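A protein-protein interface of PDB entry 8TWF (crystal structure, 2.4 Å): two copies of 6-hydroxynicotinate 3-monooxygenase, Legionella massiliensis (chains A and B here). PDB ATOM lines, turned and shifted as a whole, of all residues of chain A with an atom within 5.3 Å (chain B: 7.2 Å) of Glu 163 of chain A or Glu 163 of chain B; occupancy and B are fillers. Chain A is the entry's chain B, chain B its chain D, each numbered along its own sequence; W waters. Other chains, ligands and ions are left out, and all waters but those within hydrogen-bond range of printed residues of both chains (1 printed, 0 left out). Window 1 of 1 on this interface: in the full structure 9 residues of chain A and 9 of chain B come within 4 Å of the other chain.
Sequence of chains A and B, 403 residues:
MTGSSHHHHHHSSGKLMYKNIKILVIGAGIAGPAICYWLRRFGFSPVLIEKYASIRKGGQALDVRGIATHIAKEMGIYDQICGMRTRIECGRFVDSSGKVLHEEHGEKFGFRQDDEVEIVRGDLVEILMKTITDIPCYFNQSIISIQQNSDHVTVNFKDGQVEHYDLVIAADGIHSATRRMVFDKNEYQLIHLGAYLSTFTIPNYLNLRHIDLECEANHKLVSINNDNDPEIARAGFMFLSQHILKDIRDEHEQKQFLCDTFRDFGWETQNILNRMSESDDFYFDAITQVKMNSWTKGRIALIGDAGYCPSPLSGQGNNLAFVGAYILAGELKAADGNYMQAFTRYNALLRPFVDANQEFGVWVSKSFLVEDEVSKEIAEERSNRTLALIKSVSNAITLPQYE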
ATOM      1  N   LYS A  22      24.920 -24.130 -23.159  1.00  0.00           N
ATOM      2  CA  LYS A  22      23.565 -23.649 -22.912  1.00  0.00           C
ATOM      3  C   LYS A  22      23.481 -23.048 -21.511  1.00  0.00           C
ATOM      4  O   LYS A  22      23.709 -23.745 -20.514  1.00  0.00           O
ATOM      5  CB  LYS A  22      22.551 -24.782 -23.069  1.00  0.00           C
ATOM      6  CG  LYS A  22      22.305 -25.221 -24.507  1.00  0.00           C
ATOM      7  CD  LYS A  22      21.127 -26.191 -24.610  1.00  0.00           C
ATOM      8  CE  LYS A  22      19.796 -25.495 -24.340  1.00  0.00           C
ATOM      9  NZ  LYS A  22      18.624 -26.401 -24.518  1.00  0.00           N
ATOM     10  N   VAL A 153      21.415 -29.470 -16.178  1.00  0.00           N
ATOM     11  CA  VAL A 153      20.250 -29.059 -15.401  1.00  0.00           C
ATOM     12  C   VAL A 153      19.021 -29.197 -16.291  1.00  0.00           C
ATOM     13  O   VAL A 153      19.036 -28.761 -17.448  1.00  0.00           O
ATOM     14  CB  VAL A 153      20.401 -27.614 -14.893  1.00  0.00           C
ATOM     15  CG1 VAL A 153      19.183 -27.192 -14.076  1.00  0.00           C
ATOM     16  CG2 VAL A 153      21.679 -27.457 -14.078  1.00  0.00           C
ATOM     17  N   THR A 154      17.961 -29.803 -15.758  1.00  0.00           N
ATOM     18  CA  THR A 154      16.705 -29.984 -16.475  1.00  0.00           C
ATOM     19  C   THR A 154      15.656 -29.032 -15.917  1.00  0.00           C
ATOM     20  O   THR A 154      15.401 -29.021 -14.708  1.00  0.00           O
ATOM     21  CB  THR A 154      16.211 -31.429 -16.367  1.00  0.00           C
ATOM     22  OG1 THR A 154      17.215 -32.325 -16.861  1.00  0.00           O
ATOM     23  CG2 THR A 154      14.931 -31.615 -17.166  1.00  0.00           C
ATOM     24  N   VAL A 155      15.034 -28.252 -16.802  1.00  0.00           N
ATOM     25  CA  VAL A 155      14.115 -27.187 -16.418  1.00  0.00           C
ATOM     26  C   VAL A 155      12.767 -27.435 -17.075  1.00  0.00           C
ATOM     27  O   VAL A 155      12.679 -27.534 -18.306  1.00  0.00           O
ATOM     28  CB  VAL A 155      14.654 -25.804 -16.816  1.00  0.00           C
ATOM     29  CG1 VAL A 155      13.618 -24.737 -16.517  1.00  0.00           C
ATOM     30  CG2 VAL A 155      15.964 -25.517 -16.100  1.00  0.00           C
ATOM     31  N   PHE A 157       8.915 -26.058 -17.831  1.00  0.00           N
ATOM     32  CA  PHE A 157       8.207 -24.802 -18.013  1.00  0.00           C
ATOM     33  C   PHE A 157       6.706 -25.024 -17.918  1.00  0.00           C
ATOM     34  O   PHE A 157       6.199 -26.126 -18.143  1.00  0.00           O
ATOM     35  CB  PHE A 157       8.561 -24.161 -19.357  1.00  0.00           C
ATOM     36  CG  PHE A 157       9.977 -23.681 -19.436  1.00  0.00           C
ATOM     37  CD1 PHE A 157      10.988 -24.534 -19.841  1.00  0.00           C
ATOM     38  CD2 PHE A 157      10.300 -22.380 -19.091  1.00  0.00           C
ATOM     39  CE1 PHE A 157      12.298 -24.095 -19.907  1.00  0.00           C
ATOM     40  CE2 PHE A 157      11.607 -21.936 -19.155  1.00  0.00           C
ATOM     41  CZ  PHE A 157      12.607 -22.794 -19.565  1.00  0.00           C
ATOM     42  N   GLN A 161       7.222 -27.140 -22.042  1.00  0.00           N
ATOM     43  CA  GLN A 161       8.562 -27.381 -22.561  1.00  0.00           C
ATOM     44  C   GLN A 161       9.459 -27.987 -21.485  1.00  0.00           C
ATOM     45  O   GLN A 161       9.270 -27.770 -20.285  1.00  0.00           O
ATOM     46  CB  GLN A 161       9.170 -26.079 -23.086  1.00  0.00           C
ATOM     47  CG  GLN A 161       8.445 -25.512 -24.298  1.00  0.00           C
ATOM     48  CD  GLN A 161       9.025 -24.196 -24.772  1.00  0.00           C
ATOM     49  OE1 GLN A 161      10.179 -24.130 -25.204  1.00  0.00           O
ATOM     50  NE2 GLN A 161       8.228 -23.137 -24.692  1.00  0.00           N
ATOM     51  N   VAL A 162      10.442 -28.770 -21.935  1.00  0.00           N
ATOM     52  CA  VAL A 162      11.453 -29.372 -21.069  1.00  0.00           C
ATOM     53  C   VAL A 162      12.804 -29.203 -21.755  1.00  0.00           C
ATOM     54  O   VAL A 162      13.042 -29.800 -22.812  1.00  0.00           O
ATOM     55  CB  VAL A 162      11.183 -30.856 -20.785  1.00  0.00           C
ATOM     56  CG1 VAL A 162      12.137 -31.376 -19.712  1.00  0.00           C
ATOM     57  CG2 VAL A 162       9.737 -31.074 -20.374  1.00  0.00           C
ATOM     58  N   GLU A 163      13.691 -28.419 -21.151  1.00  0.00           N
ATOM     59  CA  GLU A 163      14.985 -28.101 -21.732  1.00  0.00           C
ATOM     60  C   GLU A 163      16.102 -28.485 -20.770  1.00  0.00           C
ATOM     61  O   GLU A 163      15.950 -28.373 -19.549  1.00  0.00           O
ATOM     62  CB  GLU A 163      15.070 -26.602 -22.068  1.00  0.00           C
ATOM     63  CG  GLU A 163      13.974 -26.102 -23.010  1.00  0.00           C
ATOM     64  CD  GLU A 163      13.946 -24.585 -23.127  1.00  0.00           C
ATOM     65  OE1 GLU A 163      14.628 -23.913 -22.323  1.00  0.00           O
ATOM     66  OE2 GLU A 163      13.241 -24.063 -24.018  1.00  0.00           O
ATOM     67  N   HIS A 164      17.220 -28.948 -21.328  1.00  0.00           N
ATOM     68  CA  HIS A 164      18.443 -29.185 -20.572  1.00  0.00           C
ATOM     69  C   HIS A 164      19.390 -28.009 -20.780  1.00  0.00           C
ATOM     70  O   HIS A 164      19.502 -27.478 -21.889  1.00  0.00           O
ATOM     71  CB  HIS A 164      19.135 -30.485 -21.000  1.00  0.00           C
ATOM     72  CG  HIS A 164      18.249 -31.689 -20.956  1.00  0.00           C
ATOM     73  ND1 HIS A 164      17.246 -31.843 -20.024  1.00  0.00           N
ATOM     74  CD2 HIS A 164      18.207 -32.793 -21.739  1.00  0.00           C
ATOM     75  CE1 HIS A 164      16.625 -32.990 -20.233  1.00  0.00           C
ATOM     76  NE2 HIS A 164      17.188 -33.587 -21.268  1.00  0.00           N
ATOM     77  N   TYR A 165      20.058 -27.600 -19.706  1.00  0.00           N
ATOM     78  CA  TYR A 165      21.041 -26.530 -19.748  1.00  0.00           C
ATOM     79  C   TYR A 165      22.305 -26.985 -19.035  1.00  0.00           C
ATOM     80  O   TYR A 165      22.251 -27.792 -18.102  1.00  0.00           O
ATOM     81  CB  TYR A 165      20.523 -25.247 -19.084  1.00  0.00           C
ATOM     82  CG  TYR A 165      19.437 -24.530 -19.851  1.00  0.00           C
ATOM     83  CD1 TYR A 165      19.755 -23.599 -20.828  1.00  0.00           C
ATOM     84  CD2 TYR A 165      18.096 -24.769 -19.585  1.00  0.00           C
ATOM     85  CE1 TYR A 165      18.770 -22.934 -21.531  1.00  0.00           C
ATOM     86  CE2 TYR A 165      17.099 -24.104 -20.282  1.00  0.00           C
ATOM     87  CZ  TYR A 165      17.445 -23.188 -21.254  1.00  0.00           C
ATOM     88  OH  TYR A 165      16.467 -22.520 -21.957  1.00  0.00           O
ATOM     89  N   LYS B  22      12.250 -17.694 -32.456  1.00  0.00           N
ATOM     90  CA  LYS B  22      12.854 -19.002 -32.200  1.00  0.00           C
ATOM     91  C   LYS B  22      12.784 -19.845 -33.471  1.00  0.00           C
ATOM     92  O   LYS B  22      11.709 -20.314 -33.861  1.00  0.00           O
ATOM     93  CB  LYS B  22      12.154 -19.711 -31.041  1.00  0.00           C
ATOM     94  CG  LYS B  22      12.444 -19.120 -29.671  1.00  0.00           C
ATOM     95  CD  LYS B  22      11.754 -19.907 -28.553  1.00  0.00           C
ATOM     96  CE  LYS B  22      12.438 -21.244 -28.295  1.00  0.00           C
ATOM     97  NZ  LYS B  22      11.790 -22.015 -27.199  1.00  0.00           N
ATOM     98  N   LEU B  24      14.496 -23.154 -35.543  1.00  0.00           N
ATOM     99  CA  LEU B  24      15.310 -24.363 -35.529  1.00  0.00           C
ATOM    100  C   LEU B  24      15.653 -24.745 -36.961  1.00  0.00           C
ATOM    101  O   LEU B  24      14.771 -24.788 -37.825  1.00  0.00           O
ATOM    102  CB  LEU B  24      14.579 -25.516 -34.837  1.00  0.00           C
ATOM    103  CG  LEU B  24      15.305 -26.865 -34.799  1.00  0.00           C
ATOM    104  CD1 LEU B  24      16.610 -26.754 -34.015  1.00  0.00           C
ATOM    105  CD2 LEU B  24      14.406 -27.949 -34.210  1.00  0.00           C
ATOM    106  N   VAL B  47      19.204 -21.785 -34.495  1.00  0.00           N
ATOM    107  CA  VAL B  47      20.001 -22.813 -33.837  1.00  0.00           C
ATOM    108  C   VAL B  47      20.071 -24.031 -34.750  1.00  0.00           C
ATOM    109  O   VAL B  47      19.060 -24.448 -35.326  1.00  0.00           O
ATOM    110  CB  VAL B  47      19.425 -23.194 -32.456  1.00  0.00           C
ATOM    111  CG1 VAL B  47      19.991 -24.523 -31.984  1.00  0.00           C
ATOM    112  CG2 VAL B  47      19.729 -22.106 -31.440  1.00  0.00           C
ATOM    113  N   ILE B  49      21.142 -28.125 -35.455  1.00  0.00           N
ATOM    114  CA  ILE B  49      21.348 -29.444 -34.874  1.00  0.00           C
ATOM    115  C   ILE B  49      21.790 -30.411 -35.966  1.00  0.00           C
ATOM    116  O   ILE B  49      21.501 -30.231 -37.153  1.00  0.00           O
ATOM    117  CB  ILE B  49      20.094 -30.006 -34.160  1.00  0.00           C
ATOM    118  CG1 ILE B  49      18.926 -30.173 -35.139  1.00  0.00           C
ATOM    119  CG2 ILE B  49      19.694 -29.116 -32.994  1.00  0.00           C
ATOM    120  CD1 ILE B  49      17.887 -31.179 -34.676  1.00  0.00           C
ATOM    121  N   TYR B 138      24.445 -28.136 -32.245  1.00  0.00           N
ATOM    122  CA  TYR B 138      24.406 -29.263 -31.317  1.00  0.00           C
ATOM    123  C   TYR B 138      24.412 -30.568 -32.102  1.00  0.00           C
ATOM    124  O   TYR B 138      23.447 -30.877 -32.811  1.00  0.00           O
ATOM    125  CB  TYR B 138      23.169 -29.183 -30.424  1.00  0.00           C
ATOM    126  CG  TYR B 138      23.036 -27.870 -29.689  1.00  0.00           C
ATOM    127  CD1 TYR B 138      23.815 -27.596 -28.573  1.00  0.00           C
ATOM    128  CD2 TYR B 138      22.131 -26.904 -30.109  1.00  0.00           C
ATOM    129  CE1 TYR B 138      23.702 -26.397 -27.899  1.00  0.00           C
ATOM    130  CE2 TYR B 138      22.010 -25.701 -29.439  1.00  0.00           C
ATOM    131  CZ  TYR B 138      22.798 -25.455 -28.333  1.00  0.00           C
ATOM    132  OH  TYR B 138      22.685 -24.261 -27.658  1.00  0.00           O
ATOM    133  N   GLN B 141      22.030 -34.685 -31.962  1.00  0.00           N
ATOM    134  CA  GLN B 141      20.666 -34.258 -31.685  1.00  0.00           C
ATOM    135  C   GLN B 141      19.772 -34.626 -32.860  1.00  0.00           C
ATOM    136  O   GLN B 141      20.143 -34.424 -34.021  1.00  0.00           O
ATOM    137  CB  GLN B 141      20.579 -32.750 -31.442  1.00  0.00           C
ATOM    138  CG  GLN B 141      21.118 -32.306 -30.111  1.00  0.00           C
ATOM    139  CD  GLN B 141      20.408 -32.965 -28.948  1.00  0.00           C
ATOM    140  OE1 GLN B 141      19.176 -33.006 -28.893  1.00  0.00           O
ATOM    141  NE2 GLN B 141      21.186 -33.501 -28.014  1.00  0.00           N
ATOM    142  N   GLN B 147       4.813 -31.743 -33.479  1.00  0.00           N
ATOM    143  CA  GLN B 147       3.456 -31.231 -33.564  1.00  0.00           C
ATOM    144  C   GLN B 147       3.548 -29.739 -33.842  1.00  0.00           C
ATOM    145  O   GLN B 147       4.569 -29.102 -33.566  1.00  0.00           O
ATOM    146  CB  GLN B 147       2.658 -31.486 -32.276  1.00  0.00           C
ATOM    147  CG  GLN B 147       2.546 -32.955 -31.883  1.00  0.00           C
ATOM    148  CD  GLN B 147       3.713 -33.440 -31.038  1.00  0.00           C
ATOM    149  OE1 GLN B 147       4.334 -32.668 -30.301  1.00  0.00           O
ATOM    150  NE2 GLN B 147       4.012 -34.730 -31.139  1.00  0.00           N
ATOM    151  N   HIS B 152       2.870 -22.115 -32.490  1.00  0.00           N
ATOM    152  CA  HIS B 152       4.247 -22.583 -32.379  1.00  0.00           C
ATOM    153  C   HIS B 152       4.333 -24.022 -32.871  1.00  0.00           C
ATOM    154  O   HIS B 152       3.320 -24.690 -33.091  1.00  0.00           O
ATOM    155  CB  HIS B 152       4.757 -22.474 -30.936  1.00  0.00           C
ATOM    156  CG  HIS B 152       3.977 -23.299 -29.961  1.00  0.00           C
ATOM    157  ND1 HIS B 152       4.405 -24.531 -29.517  1.00  0.00           N
ATOM    158  CD2 HIS B 152       2.787 -23.074 -29.356  1.00  0.00           C
ATOM    159  CE1 HIS B 152       3.514 -25.028 -28.677  1.00  0.00           C
ATOM    160  NE2 HIS B 152       2.523 -24.163 -28.563  1.00  0.00           N
ATOM    161  N   VAL B 153       5.567 -24.488 -33.040  1.00  0.00           N
ATOM    162  CA  VAL B 153       5.864 -25.866 -33.413  1.00  0.00           C
ATOM    163  C   VAL B 153       6.488 -26.560 -32.209  1.00  0.00           C
ATOM    164  O   VAL B 153       7.430 -26.036 -31.604  1.00  0.00           O
ATOM    165  CB  VAL B 153       6.807 -25.923 -34.628  1.00  0.00           C
ATOM    166  CG1 VAL B 153       7.066 -27.364 -35.030  1.00  0.00           C
ATOM    167  CG2 VAL B 153       6.231 -25.110 -35.794  1.00  0.00           C
ATOM    168  N   THR B 154       5.966 -27.736 -31.861  1.00  0.00           N
ATOM    169  CA  THR B 154       6.475 -28.522 -30.740  1.00  0.00           C
ATOM    170  C   THR B 154       7.439 -29.575 -31.282  1.00  0.00           C
ATOM    171  O   THR B 154       7.025 -30.512 -31.972  1.00  0.00           O
ATOM    172  CB  THR B 154       5.335 -29.175 -29.958  1.00  0.00           C
ATOM    173  OG1 THR B 154       4.421 -28.170 -29.501  1.00  0.00           O
ATOM    174  CG2 THR B 154       5.872 -29.937 -28.748  1.00  0.00           C
ATOM    175  N   VAL B 155       8.721 -29.424 -30.959  1.00  0.00           N
ATOM    176  CA  VAL B 155       9.771 -30.336 -31.394  1.00  0.00           C
ATOM    177  C   VAL B 155      10.208 -31.164 -30.193  1.00  0.00           C
ATOM    178  O   VAL B 155      10.669 -30.615 -29.184  1.00  0.00           O
ATOM    179  CB  VAL B 155      10.959 -29.575 -32.001  1.00  0.00           C
ATOM    180  CG1 VAL B 155      12.087 -30.534 -32.317  1.00  0.00           C
ATOM    181  CG2 VAL B 155      10.517 -28.814 -33.247  1.00  0.00           C
ATOM    182  N   ASN B 156      10.070 -32.480 -30.302  1.00  0.00           N
ATOM    183  CA  ASN B 156      10.433 -33.404 -29.236  1.00  0.00           C
ATOM    184  C   ASN B 156      11.720 -34.119 -29.616  1.00  0.00           C
ATOM    185  O   ASN B 156      11.813 -34.706 -30.698  1.00  0.00           O
ATOM    186  CB  ASN B 156       9.305 -34.401 -28.984  1.00  0.00           C
ATOM    187  CG  ASN B 156       7.991 -33.713 -28.672  1.00  0.00           C
ATOM    188  OD1 ASN B 156       7.811 -33.171 -27.586  1.00  0.00           O
ATOM    189  ND2 ASN B 156       7.071 -33.717 -29.632  1.00  0.00           N
ATOM    190  N   PHE B 157      12.701 -34.076 -28.721  1.00  0.00           N
ATOM    191  CA  PHE B 157      14.060 -34.474 -29.046  1.00  0.00           C
ATOM    192  C   PHE B 157      14.380 -35.877 -28.542  1.00  0.00           C
ATOM    193  O   PHE B 157      13.674 -36.459 -27.718  1.00  0.00           O
ATOM    194  CB  PHE B 157      15.058 -33.463 -28.473  1.00  0.00           C
ATOM    195  CG  PHE B 157      15.188 -32.216 -29.297  1.00  0.00           C
ATOM    196  CD1 PHE B 157      16.041 -32.182 -30.388  1.00  0.00           C
ATOM    197  CD2 PHE B 157      14.452 -31.084 -28.991  1.00  0.00           C
ATOM    198  CE1 PHE B 157      16.163 -31.041 -31.154  1.00  0.00           C
ATOM    199  CE2 PHE B 157      14.570 -29.938 -29.753  1.00  0.00           C
ATOM    200  CZ  PHE B 157      15.426 -29.918 -30.837  1.00  0.00           C
ATOM    201  N   ASP B 159      16.946 -36.825 -26.722  1.00  0.00           N
ATOM    202  CA  ASP B 159      17.423 -36.832 -25.347  1.00  0.00           C
ATOM    203  C   ASP B 159      16.347 -36.436 -24.343  1.00  0.00           C
ATOM    204  O   ASP B 159      16.656 -36.266 -23.159  1.00  0.00           O
ATOM    205  CB  ASP B 159      18.634 -35.902 -25.207  1.00  0.00           C
ATOM    206  CG  ASP B 159      18.330 -34.474 -25.624  1.00  0.00           C
ATOM    207  OD1 ASP B 159      17.155 -34.169 -25.918  1.00  0.00           O
ATOM    208  OD2 ASP B 159      19.273 -33.654 -25.659  1.00  0.00           O
ATOM    209  N   GLY B 160      15.101 -36.283 -24.781  1.00  0.00           N
ATOM    210  CA  GLY B 160      13.997 -36.038 -23.880  1.00  0.00           C
ATOM    211  C   GLY B 160      13.543 -34.601 -23.750  1.00  0.00           C
ATOM    212  O   GLY B 160      12.707 -34.314 -22.885  1.00  0.00           O
ATOM    213  N   GLN B 161      14.046 -33.697 -24.581  1.00  0.00           N
ATOM    214  CA  GLN B 161      13.665 -32.296 -24.499  1.00  0.00           C
ATOM    215  C   GLN B 161      12.415 -32.039 -25.329  1.00  0.00           C
ATOM    216  O   GLN B 161      12.171 -32.693 -26.347  1.00  0.00           O
ATOM    217  CB  GLN B 161      14.810 -31.396 -24.966  1.00  0.00           C
ATOM    218  CG  GLN B 161      16.026 -31.432 -24.054  1.00  0.00           C
ATOM    219  CD  GLN B 161      17.141 -30.519 -24.526  1.00  0.00           C
ATOM    220  OE1 GLN B 161      17.086 -29.303 -24.338  1.00  0.00           O
ATOM    221  NE2 GLN B 161      18.161 -31.102 -25.143  1.00  0.00           N
ATOM    222  N   VAL B 162      11.605 -31.097 -24.855  1.00  0.00           N
ATOM    223  CA  VAL B 162      10.417 -30.626 -25.556  1.00  0.00           C
ATOM    224  C   VAL B 162      10.546 -29.115 -25.672  1.00  0.00           C
ATOM    225  O   VAL B 162      10.600 -28.416 -24.651  1.00  0.00           O
ATOM    226  CB  VAL B 162       9.119 -31.005 -24.826  1.00  0.00           C
ATOM    227  CG1 VAL B 162       7.898 -30.564 -25.631  1.00  0.00           C
ATOM    228  CG2 VAL B 162       9.071 -32.500 -24.555  1.00  0.00           C
ATOM    229  N   GLU B 163      10.603 -28.612 -26.902  1.00  0.00           N
ATOM    230  CA  GLU B 163      10.829 -27.197 -27.155  1.00  0.00           C
ATOM    231  C   GLU B 163       9.776 -26.665 -28.116  1.00  0.00           C
ATOM    232  O   GLU B 163       9.298 -27.379 -29.002  1.00  0.00           O
ATOM    233  CB  GLU B 163      12.249 -26.956 -27.715  1.00  0.00           C
ATOM    234  CG  GLU B 163      13.365 -27.325 -26.728  1.00  0.00           C
ATOM    235  CD  GLU B 163      14.770 -27.242 -27.324  1.00  0.00           C
ATOM    236  OE1 GLU B 163      14.900 -27.019 -28.549  1.00  0.00           O
ATOM    237  OE2 GLU B 163      15.748 -27.407 -26.558  1.00  0.00           O
ATOM    238  N   HIS B 164       9.409 -25.402 -27.916  1.00  0.00           N
ATOM    239  CA  HIS B 164       8.478 -24.696 -28.784  1.00  0.00           C
ATOM    240  C   HIS B 164       9.260 -23.734 -29.671  1.00  0.00           C
ATOM    241  O   HIS B 164      10.159 -23.032 -29.199  1.00  0.00           O
ATOM    242  CB  HIS B 164       7.434 -23.931 -27.961  1.00  0.00           C
ATOM    243  CG  HIS B 164       6.569 -24.807 -27.106  1.00  0.00           C
ATOM    244  ND1 HIS B 164       5.589 -24.301 -26.278  1.00  0.00           N
ATOM    245  CD2 HIS B 164       6.533 -26.153 -26.951  1.00  0.00           C
ATOM    246  CE1 HIS B 164       4.989 -25.296 -25.649  1.00  0.00           C
ATOM    247  NE2 HIS B 164       5.542 -26.430 -26.039  1.00  0.00           N
ATOM    248  N   TYR B 165       8.918 -23.708 -30.962  1.00  0.00           N
ATOM    249  CA  TYR B 165       9.603 -22.872 -31.939  1.00  0.00           C
ATOM    250  C   TYR B 165       8.586 -22.093 -32.757  1.00  0.00           C
ATOM    251  O   TYR B 165       7.489 -22.578 -33.046  1.00  0.00           O
ATOM    252  CB  TYR B 165      10.497 -23.701 -32.891  1.00  0.00           C
ATOM    253  CG  TYR B 165      11.810 -24.128 -32.274  1.00  0.00           C
ATOM    254  CD1 TYR B 165      12.907 -23.276 -32.273  1.00  0.00           C
ATOM    255  CD2 TYR B 165      11.951 -25.378 -31.689  1.00  0.00           C
ATOM    256  CE1 TYR B 165      14.106 -23.657 -31.702  1.00  0.00           C
ATOM    257  CE2 TYR B 165      13.146 -25.770 -31.119  1.00  0.00           C
ATOM    258  CZ  TYR B 165      14.218 -24.907 -31.126  1.00  0.00           C
ATOM    259  OH  TYR B 165      15.408 -25.297 -30.557  1.00  0.00           O
HETATM  260  O   HOH W   1      13.013 -21.439 -24.133  1.00  0.00           O
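The backbone carbonyl oxygen (O) of Val 162 of chain B sits at hydrogen-bond distance from the backbone NH (N) of Val 162 of chain A, 2.7 Å away.
The side-chain amino group (NZ) of Lys 22 of chain A is in salt-bridge range of the side-chain carboxylate (OE2) of Glu 163 of chain B, 3.7 Å away.
The backbone NH of His 164 of chain B is in hydrogen-bond range of the side-chain amide oxygen of Gln 161 of chain A, 3.1 Å away.
N of His 164 of chain A is in hydrogen-bond range of OE1 of Gln 161 of chain B (3.0 Å).
The side-chain amino group of Lys 22 of chain B lies within hydrogen-bond range of the side-chain amide oxygen of Gln 161 of chain A, 3.3 Å away.
The side-chain amino group (NZ) of Lys 22 of chain A sits at hydrogen-bond distance from the side-chain amide oxygen (OE1) of Gln 161 of chain B, 3.3 Å away.
The backbone carbonyl oxygen (O) of Asp 159 of chain B lies within hydrogen-bond range of a ring nitrogen (NE2) of His 164 of chain A (3.3 Å).
The backbone carbonyl oxygen (O) of Glu 163 of chain B sits at hydrogen-bond distance from the backbone NH (N) of Val 155 of chain B (2.9 Å).
The side-chain carboxylate (OE2) of Glu 163 of chain B sits close to the side-chain amide oxygen (OE1) of Gln 161 of chain B (3.2 Å).
The backbone carbonyl oxygen of His 164 of chain A lies within hydrogen-bond range of the side-chain amino group of Lys 22 of chain A (3.0 Å).
ND1 of His 164 of chain B sits close to ND1 of His 152 of chain B, at 3.5 Å.
O of Glu 163 of chain A lies within hydrogen-bond range of N of Val 155 of chain A (2.9 Å).
NE2 of Gln 141 of chain B is in hydrogen-bond range of OD2 of Asp 159 of chain B, 3.0 Å away.
CG of Lys 22 of chain A touches OH of Tyr 138 of chain B (3.3 Å).
Gln 161 of chain A touches Val 162 of chain B.
Glu 163 of chain B touches Gln 161 of chain A (CA to OE1, 3.7 Å).
Gln 161 of chain B touches Val 162 of chain A (CA to O, 3.1 Å).
Gln 161 of chain B touches Glu 163 of chain A (OE1 to CA, 3.6 Å).
Glu 163 of chain A touches Glu 163 of chain B.
Glu 163 of chain A touches two residues of chain B.
Glu 163 of chain B touches just these residues of chain A: Lys 22, Gln 161 and Glu 163.
Printed residues of chain B within 4 Å of Lys 22 of chain A: Tyr 138 (3.3 Å), Gln 161 (3.3 Å) and Glu 163 (3.7 Å).
Of the printed residues of chain B, Gln 161 of chain A touches Lys 22 (3.3 Å), Val 162 (3.1 Å), Glu 163 (3.7 Å) and His 164 (3.1 Å).
Of the printed residues of chain A, Asp 159 of chain B touches His 164.
Of the printed residues of chain A, Lys 22 of chain B touches Gln 161 (3.3 Å).
Printed residues of chain B within 4 Å of His 164 of chain A: Asp 159 and Gln 161.
The nearest residue of chain A that does not touch Glu 163 of chain B is Val 162 of chain A (4.6 Å).
Of the 20 printed residues of chain B, 7 touch a printed residue of chain A.
Printed residues of chain B that touch a printed residue of chain A: Lys 22, Tyr 138, Asp 159, Gln 161, Val 162, Glu 163 and His 164.
Of the 10 printed residues of chain A, 5 touch a printed residue of chain B.
Among the printed residues, Asp or Glu carboxylates within 4 Å of a Lys or Arg side-chain nitrogen of the other chain: Lys 22 of chain A with Glu 163 of chain B (3.7 Å).
Gln 161 of chain A touches Glu 163 of chain B, and with the chains exchanged Glu 163 of chain A touches Gln 161 of chain B.
Gln 161 of chain A touches His 164 of chain B, and with the chains exchanged His 164 of chain A touches Gln 161 of chain B.
Val 162 of chain B touches its own counterpart, Val 162 of chain A.
Glu 163 of chain B touches its own counterpart, Glu 163 of chain A.
Of the 13 pairs that touch across the chains among the printed residues, 10 have their exchanged pair printed and touching as well.
Water W1 bridges the side-chain carboxylate (OE2) of Glu 163 of chain A (2.6 Å) and the side-chain amino group (NZ) of Lys 22 of chain B (3.4 Å).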
